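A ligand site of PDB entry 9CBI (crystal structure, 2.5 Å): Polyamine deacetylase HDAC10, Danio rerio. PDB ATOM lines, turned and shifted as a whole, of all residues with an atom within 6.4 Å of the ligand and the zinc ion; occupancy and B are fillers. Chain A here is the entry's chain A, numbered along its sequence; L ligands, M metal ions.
OE2 of Glu 274 is in salt-bridge range of N1 of the ligand (2.7 Å).
OH of Tyr 307 is in hydrogen-bond range of O1 of the ligand (2.8 Å).
NE2 of His 136 sits close to S1 of the ligand.
OD1 of Asp 267 lies within hydrogen-bond range of N of Val 175, at 3.0 Å.
The side-chain carboxylate of Asp 174 is in hydrogen-bond range of the backbone NH of Gly 305.
A ring nitrogen (NE2) of His 137 is in hydrogen-bond range of a ring nitrogen (NE2) of His 136, 3.0 Å away.
OE1 of Glu 304 is in hydrogen-bond range of N of His 136.
N of His 136 sits at hydrogen-bond distance from SG of Cys 147, 3.8 Å away.
N of Phe 146 is in hydrogen-bond range of O of Ala 94, at 2.9 Å.
The backbone carbonyl oxygen of Asn 93 sits at hydrogen-bond distance from the backbone NH of Gly 145, 3.3 Å away.
NE1 of Trp 205 lies within hydrogen-bond range of OD1 of Asn 93 (2.8 Å).
Residues that only touch the ligand: Glu 24, Ala 94, His 137, Gly 145, Phe 146, Trp 205 and Gly 305.
Hydrophobic or aromatic side chains within 4 Å of the ligand: Ala 94, His 137, Phe 146, His 176, Trp 205 and Tyr 307.
Within 4 Å of the zinc ion: Asp 174, His 176 and Asp 267.
The side-chain carboxylate (OD2) of Asp 267 is bound to the zinc ion (2.0 Å).
The zinc ion is bound by OD1 of Asp 174, 2.2 Å away.
ND1 of His 176 is bound to the zinc ion (2.3 Å).
The zinc ion is bound by S1 of the ligand (2.4 Å).
The zinc ion has four donor atoms within binding distance.
Slightly farther from the zinc ion lies OD2 of Asp 174 (2.8 Å).
Slightly farther from the zinc ion lies O1 of the ligand (2.8 Å).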
ATOM      1  N   GLU A  24      25.749  28.694  29.884  1.00  0.00           N
ATOM      2  CA  GLU A  24      25.600  27.863  28.693  1.00  0.00           C
ATOM      3  C   GLU A  24      24.381  26.948  28.790  1.00  0.00           C
ATOM      4  O   GLU A  24      23.813  26.570  27.755  1.00  0.00           O
ATOM      5  CB  GLU A  24      26.864  27.032  28.469  1.00  0.00           C
ATOM      6  CG  GLU A  24      27.417  27.114  27.052  1.00  0.00           C
ATOM      7  CD  GLU A  24      28.725  26.359  26.892  1.00  0.00           C
ATOM      8  N   CYS A  25      23.964  26.575  30.004  1.00  0.00           N
ATOM      9  CA  CYS A  25      22.878  25.620  30.203  1.00  0.00           C
ATOM     10  C   CYS A  25      21.641  26.220  30.842  1.00  0.00           C
ATOM     11  O   CYS A  25      20.688  25.481  31.122  1.00  0.00           O
ATOM     12  CB  CYS A  25      23.373  24.446  31.061  1.00  0.00           C
ATOM     13  SG  CYS A  25      24.810  23.566  30.422  1.00  0.00           S
ATOM     14  N   ILE A  27      19.205  27.673  29.724  1.00  0.00           N
ATOM     15  CA  ILE A  27      17.974  27.597  28.934  1.00  0.00           C
ATOM     16  C   ILE A  27      17.247  26.280  29.137  1.00  0.00           C
ATOM     17  O   ILE A  27      16.009  26.230  29.086  1.00  0.00           O
ATOM     18  CB  ILE A  27      18.274  27.834  27.451  1.00  0.00           C
ATOM     19  CG1 ILE A  27      19.384  26.896  26.974  1.00  0.00           C
ATOM     20  CG2 ILE A  27      18.653  29.286  27.205  1.00  0.00           C
ATOM     21  CD1 ILE A  27      19.671  26.985  25.495  1.00  0.00           C
ATOM     22  N   ASN A  93      31.077  18.699  27.816  1.00  0.00           N
ATOM     23  CA  ASN A  93      30.855  19.971  27.132  1.00  0.00           C
ATOM     24  C   ASN A  93      29.376  20.302  27.075  1.00  0.00           C
ATOM     25  O   ASN A  93      28.586  19.526  26.520  1.00  0.00           O
ATOM     26  CB  ASN A  93      31.455  19.933  25.725  1.00  0.00           C
ATOM     27  CG  ASN A  93      31.340  21.273  25.012  1.00  0.00           C
ATOM     28  OD1 ASN A  93      30.516  21.444  24.117  1.00  0.00           O
ATOM     29  ND2 ASN A  93      32.172  22.234  25.411  1.00  0.00           N
ATOM     30  N   ALA A  94      29.002  21.449  27.646  1.00  0.00           N
ATOM     31  CA  ALA A  94      27.646  22.004  27.534  1.00  0.00           C
ATOM     32  C   ALA A  94      26.596  21.058  28.109  1.00  0.00           C
ATOM     33  O   ALA A  94      25.517  20.883  27.548  1.00  0.00           O
ATOM     34  CB  ALA A  94      27.308  22.375  26.088  1.00  0.00           C
ATOM     35  N   PRO A 134      17.221  15.692  26.175  1.00  0.00           N
ATOM     36  CA  PRO A 134      17.316  15.318  24.753  1.00  0.00           C
ATOM     37  C   PRO A 134      18.429  14.313  24.528  1.00  0.00           C
ATOM     38  O   PRO A 134      19.106  13.912  25.479  1.00  0.00           O
ATOM     39  CB  PRO A 134      17.613  16.657  24.068  1.00  0.00           C
ATOM     40  CG  PRO A 134      18.277  17.471  25.124  1.00  0.00           C
ATOM     41  CD  PRO A 134      17.609  17.088  26.414  1.00  0.00           C
ATOM     42  N   HIS A 136      20.215  13.744  20.888  1.00  0.00           N
ATOM     43  CA  HIS A 136      20.918  13.638  19.612  1.00  0.00           C
ATOM     44  C   HIS A 136      22.371  14.101  19.671  1.00  0.00           C
ATOM     45  O   HIS A 136      23.111  13.855  18.707  1.00  0.00           O
ATOM     46  CB  HIS A 136      20.162  14.382  18.509  1.00  0.00           C
ATOM     47  CG  HIS A 136      20.142  15.873  18.667  1.00  0.00           C
ATOM     48  ND1 HIS A 136      19.975  16.731  17.602  1.00  0.00           N
ATOM     49  CD2 HIS A 136      20.237  16.664  19.769  1.00  0.00           C
ATOM     50  CE1 HIS A 136      19.982  17.978  18.034  1.00  0.00           C
ATOM     51  NE2 HIS A 136      20.144  17.966  19.338  1.00  0.00           N
ATOM     52  N   HIS A 137      22.812  14.729  20.750  1.00  0.00           N
ATOM     53  CA  HIS A 137      24.210  15.121  20.861  1.00  0.00           C
ATOM     54  C   HIS A 137      25.068  14.117  21.627  1.00  0.00           C
ATOM     55  O   HIS A 137      26.288  14.099  21.430  1.00  0.00           O
ATOM     56  CB  HIS A 137      24.342  16.489  21.544  1.00  0.00           C
ATOM     57  CG  HIS A 137      23.826  17.621  20.731  1.00  0.00           C
ATOM     58  ND1 HIS A 137      24.406  18.004  19.534  1.00  0.00           N
ATOM     59  CD2 HIS A 137      22.794  18.469  20.936  1.00  0.00           C
ATOM     60  CE1 HIS A 137      23.734  19.037  19.035  1.00  0.00           C
ATOM     61  NE2 HIS A 137      22.757  19.345  19.874  1.00  0.00           N
ATOM     62  N   ASN A 144      26.784  15.264  26.049  1.00  0.00           N
ATOM     63  CA  ASN A 144      27.095  16.420  25.216  1.00  0.00           C
ATOM     64  C   ASN A 144      25.817  17.194  24.921  1.00  0.00           C
ATOM     65  O   ASN A 144      24.759  16.591  24.707  1.00  0.00           O
ATOM     66  CB  ASN A 144      27.762  15.982  23.913  1.00  0.00           C
ATOM     67  CG  ASN A 144      28.356  17.132  23.139  1.00  0.00           C
ATOM     68  OD1 ASN A 144      27.722  17.687  22.241  1.00  0.00           O
ATOM     69  ND2 ASN A 144      29.594  17.496  23.474  1.00  0.00           N
ATOM     70  N   GLY A 145      25.923  18.522  24.904  1.00  0.00           N
ATOM     71  CA  GLY A 145      24.826  19.399  24.535  1.00  0.00           C
ATOM     72  C   GLY A 145      23.486  19.075  25.160  1.00  0.00           C
ATOM     73  O   GLY A 145      22.521  18.765  24.453  1.00  0.00           O
ATOM     74  N   PHE A 146      23.414  19.117  26.493  1.00  0.00           N
ATOM     75  CA  PHE A 146      22.244  18.836  27.312  1.00  0.00           C
ATOM     76  C   PHE A 146      21.792  17.376  27.231  1.00  0.00           C
ATOM     77  O   PHE A 146      20.756  17.038  27.813  1.00  0.00           O
ATOM     78  CB  PHE A 146      21.029  19.716  26.968  1.00  0.00           C
ATOM     79  CG  PHE A 146      21.332  21.181  26.896  1.00  0.00           C
ATOM     80  CD1 PHE A 146      22.378  21.736  27.628  1.00  0.00           C
ATOM     81  CD2 PHE A 146      20.566  22.021  26.104  1.00  0.00           C
ATOM     82  CE1 PHE A 146      22.648  23.089  27.553  1.00  0.00           C
ATOM     83  CE2 PHE A 146      20.830  23.367  26.026  1.00  0.00           C
ATOM     84  CZ  PHE A 146      21.876  23.908  26.758  1.00  0.00           C
ATOM     85  N   CYS A 147      22.515  16.512  26.530  1.00  0.00           N
ATOM     86  CA  CYS A 147      22.087  15.138  26.295  1.00  0.00           C
ATOM     87  C   CYS A 147      22.935  14.169  27.101  1.00  0.00           C
ATOM     88  O   CYS A 147      24.156  14.346  27.233  1.00  0.00           O
ATOM     89  CB  CYS A 147      22.163  14.793  24.811  1.00  0.00           C
ATOM     90  SG  CYS A 147      21.271  15.943  23.746  1.00  0.00           S
ATOM     91  N   ASP A 174      15.998  19.719  14.613  1.00  0.00           N
ATOM     92  CA  ASP A 174      16.585  20.564  15.636  1.00  0.00           C
ATOM     93  C   ASP A 174      17.596  21.505  14.989  1.00  0.00           C
ATOM     94  O   ASP A 174      18.224  21.185  13.975  1.00  0.00           O
ATOM     95  CB  ASP A 174      17.255  19.695  16.713  1.00  0.00           C
ATOM     96  CG  ASP A 174      17.670  20.492  17.933  1.00  0.00           C
ATOM     97  OD1 ASP A 174      18.554  21.372  17.820  1.00  0.00           O
ATOM     98  OD2 ASP A 174      17.116  20.229  19.022  1.00  0.00           O
ATOM     99  N   VAL A 175      17.758  22.696  15.576  1.00  0.00           N
ATOM    100  CA  VAL A 175      18.655  23.688  14.999  1.00  0.00           C
ATOM    101  C   VAL A 175      20.118  23.335  15.180  1.00  0.00           C
ATOM    102  O   VAL A 175      20.980  23.960  14.555  1.00  0.00           O
ATOM    103  CB  VAL A 175      18.373  25.088  15.589  1.00  0.00           C
ATOM    104  CG1 VAL A 175      19.209  25.316  16.850  1.00  0.00           C
ATOM    105  CG2 VAL A 175      18.645  26.169  14.542  1.00  0.00           C
ATOM    106  N   HIS A 176      20.425  22.350  16.022  1.00  0.00           N
ATOM    107  CA  HIS A 176      21.792  21.886  16.205  1.00  0.00           C
ATOM    108  C   HIS A 176      22.007  20.574  15.455  1.00  0.00           C
ATOM    109  O   HIS A 176      21.074  19.820  15.176  1.00  0.00           O
ATOM    110  CB  HIS A 176      22.100  21.684  17.693  1.00  0.00           C
ATOM    111  CG  HIS A 176      21.980  22.936  18.505  1.00  0.00           C
ATOM    112  ND1 HIS A 176      20.795  23.359  19.068  1.00  0.00           N
ATOM    113  CD2 HIS A 176      22.912  23.867  18.850  1.00  0.00           C
ATOM    114  CE1 HIS A 176      20.987  24.479  19.723  1.00  0.00           C
ATOM    115  NE2 HIS A 176      22.267  24.820  19.607  1.00  0.00           N
ATOM    116  N   PHE A 204      29.430  28.123  14.684  1.00  0.00           N
ATOM    117  CA  PHE A 204      28.384  27.887  15.666  1.00  0.00           C
ATOM    118  C   PHE A 204      28.528  26.490  16.272  1.00  0.00           C
ATOM    119  O   PHE A 204      28.970  25.547  15.611  1.00  0.00           O
ATOM    120  CB  PHE A 204      26.992  28.038  15.046  1.00  0.00           C
ATOM    121  CG  PHE A 204      25.878  28.001  16.054  1.00  0.00           C
ATOM    122  CD1 PHE A 204      25.664  29.085  16.891  1.00  0.00           C
ATOM    123  CD2 PHE A 204      25.046  26.900  16.156  1.00  0.00           C
ATOM    124  CE1 PHE A 204      24.636  29.068  17.827  1.00  0.00           C
ATOM    125  CE2 PHE A 204      24.015  26.877  17.080  1.00  0.00           C
ATOM    126  CZ  PHE A 204      23.819  27.960  17.914  1.00  0.00           C
ATOM    127  N   TRP A 205      28.146  26.391  17.545  1.00  0.00           N
ATOM    128  CA  TRP A 205      28.278  25.142  18.277  1.00  0.00           C
ATOM    129  C   TRP A 205      27.502  24.029  17.563  1.00  0.00           C
ATOM    130  O   TRP A 205      26.389  24.257  17.087  1.00  0.00           O
ATOM    131  CB  TRP A 205      27.750  25.320  19.705  1.00  0.00           C
ATOM    132  CG  TRP A 205      28.103  24.191  20.610  1.00  0.00           C
ATOM    133  CD1 TRP A 205      29.185  24.108  21.433  1.00  0.00           C
ATOM    134  CD2 TRP A 205      27.371  22.967  20.778  1.00  0.00           C
ATOM    135  NE1 TRP A 205      29.175  22.905  22.103  1.00  0.00           N
ATOM    136  CE2 TRP A 205      28.067  22.191  21.714  1.00  0.00           C
ATOM    137  CE3 TRP A 205      26.190  22.470  20.217  1.00  0.00           C
ATOM    138  CZ2 TRP A 205      27.629  20.937  22.109  1.00  0.00           C
ATOM    139  CZ3 TRP A 205      25.752  21.216  20.611  1.00  0.00           C
ATOM    140  CH2 TRP A 205      26.472  20.460  21.547  1.00  0.00           C
ATOM    141  N   GLY A 265      13.455  18.800  17.525  1.00  0.00           N
ATOM    142  CA  GLY A 265      13.965  19.925  18.264  1.00  0.00           C
ATOM    143  C   GLY A 265      13.384  21.204  17.696  1.00  0.00           C
ATOM    144  O   GLY A 265      13.560  21.504  16.519  1.00  0.00           O
ATOM    145  N   ASP A 267      14.056  24.312  18.631  1.00  0.00           N
ATOM    146  CA  ASP A 267      14.893  25.495  18.662  1.00  0.00           C
ATOM    147  C   ASP A 267      15.160  26.058  17.274  1.00  0.00           C
ATOM    148  O   ASP A 267      15.841  27.091  17.159  1.00  0.00           O
ATOM    149  CB  ASP A 267      16.218  25.196  19.372  1.00  0.00           C
ATOM    150  CG  ASP A 267      16.835  23.886  18.940  1.00  0.00           C
ATOM    151  OD1 ASP A 267      16.251  23.209  18.061  1.00  0.00           O
ATOM    152  OD2 ASP A 267      17.890  23.524  19.489  1.00  0.00           O
ATOM    153  N   GLU A 274      18.450  30.327  20.961  1.00  0.00           N
ATOM    154  CA  GLU A 274      19.617  29.527  20.608  1.00  0.00           C
ATOM    155  C   GLU A 274      19.763  29.330  19.100  1.00  0.00           C
ATOM    156  O   GLU A 274      20.890  29.332  18.589  1.00  0.00           O
ATOM    157  CB  GLU A 274      19.556  28.162  21.299  1.00  0.00           C
ATOM    158  CG  GLU A 274      20.845  27.378  21.250  1.00  0.00           C
ATOM    159  CD  GLU A 274      21.973  28.037  22.029  1.00  0.00           C
ATOM    160  OE1 GLU A 274      21.675  28.796  22.970  1.00  0.00           O
ATOM    161  OE2 GLU A 274      23.155  27.781  21.695  1.00  0.00           O
ATOM    162  N   GLU A 304      13.505  17.128  21.222  1.00  0.00           N
ATOM    163  CA  GLU A 304      14.914  17.448  21.447  1.00  0.00           C
ATOM    164  C   GLU A 304      15.023  18.831  22.076  1.00  0.00           C
ATOM    165  O   GLU A 304      14.652  19.016  23.235  1.00  0.00           O
ATOM    166  CB  GLU A 304      15.705  17.368  20.145  1.00  0.00           C
ATOM    167  CG  GLU A 304      15.674  16.005  19.462  1.00  0.00           C
ATOM    168  CD  GLU A 304      16.678  15.020  20.052  1.00  0.00           C
ATOM    169  OE1 GLU A 304      17.485  15.438  20.898  1.00  0.00           O
ATOM    170  OE2 GLU A 304      16.652  13.830  19.667  1.00  0.00           O
ATOM    171  N   GLY A 305      15.509  19.806  21.309  1.00  0.00           N
ATOM    172  CA  GLY A 305      15.665  21.162  21.795  1.00  0.00           C
ATOM    173  C   GLY A 305      14.381  21.962  21.693  1.00  0.00           C
ATOM    174  O   GLY A 305      13.286  21.444  21.464  1.00  0.00           O
ATOM    175  N   GLY A 306      14.534  23.272  21.883  1.00  0.00           N
ATOM    176  CA  GLY A 306      13.413  24.195  21.908  1.00  0.00           C
ATOM    177  C   GLY A 306      13.284  24.882  23.250  1.00  0.00           C
ATOM    178  O   GLY A 306      12.923  24.241  24.248  1.00  0.00           O
ATOM    179  N   TYR A 307      13.568  26.183  23.301  1.00  0.00           N
ATOM    180  CA  TYR A 307      13.761  26.864  24.577  1.00  0.00           C
ATOM    181  C   TYR A 307      12.975  28.152  24.760  1.00  0.00           C
ATOM    182  O   TYR A 307      12.945  28.677  25.884  1.00  0.00           O
ATOM    183  CB  TYR A 307      15.252  27.133  24.805  1.00  0.00           C
ATOM    184  CG  TYR A 307      16.052  25.872  24.628  1.00  0.00           C
ATOM    185  CD1 TYR A 307      16.093  24.912  25.637  1.00  0.00           C
ATOM    186  CD2 TYR A 307      16.723  25.596  23.448  1.00  0.00           C
ATOM    187  CE1 TYR A 307      16.793  23.738  25.483  1.00  0.00           C
ATOM    188  CE2 TYR A 307      17.437  24.429  23.277  1.00  0.00           C
ATOM    189  CZ  TYR A 307      17.465  23.504  24.303  1.00  0.00           C
ATOM    190  OH  TYR A 307      18.169  22.330  24.139  1.00  0.00           O
HETATM  191  C1  LIG L   1      21.081  21.051  22.223  1.00  0.00           C
HETATM  192  C2  LIG L   1      21.060  22.563  22.435  1.00  0.00           C
HETATM  193  C3  LIG L   1      22.296  23.294  22.902  1.00  0.00           C
HETATM  194  C4  LIG L   1      23.537  22.608  23.007  1.00  0.00           C
HETATM  195  C5  LIG L   1      24.700  23.263  23.441  1.00  0.00           C
HETATM  196  C6  LIG L   1      24.714  24.617  23.811  1.00  0.00           C
HETATM  197  C7  LIG L   1      25.980  25.319  24.279  1.00  0.00           C
HETATM  198  C8  LIG L   1      26.622  26.370  23.318  1.00  0.00           C
HETATM  199  C9  LIG L   1      23.484  25.281  23.699  1.00  0.00           C
HETATM  200  C10 LIG L   1      22.314  24.633  23.262  1.00  0.00           C
HETATM  201  N1  LIG L   1      25.670  27.283  22.675  1.00  0.00           N
HETATM  202  O1  LIG L   1      20.045  23.161  22.233  1.00  0.00           O
HETATM  203  S1  LIG L   1      19.482  20.430  21.532  1.00  0.00           S
HETATM  204 ZN    ZN M   1      19.104  22.008  19.831  1.00  0.00          ZN
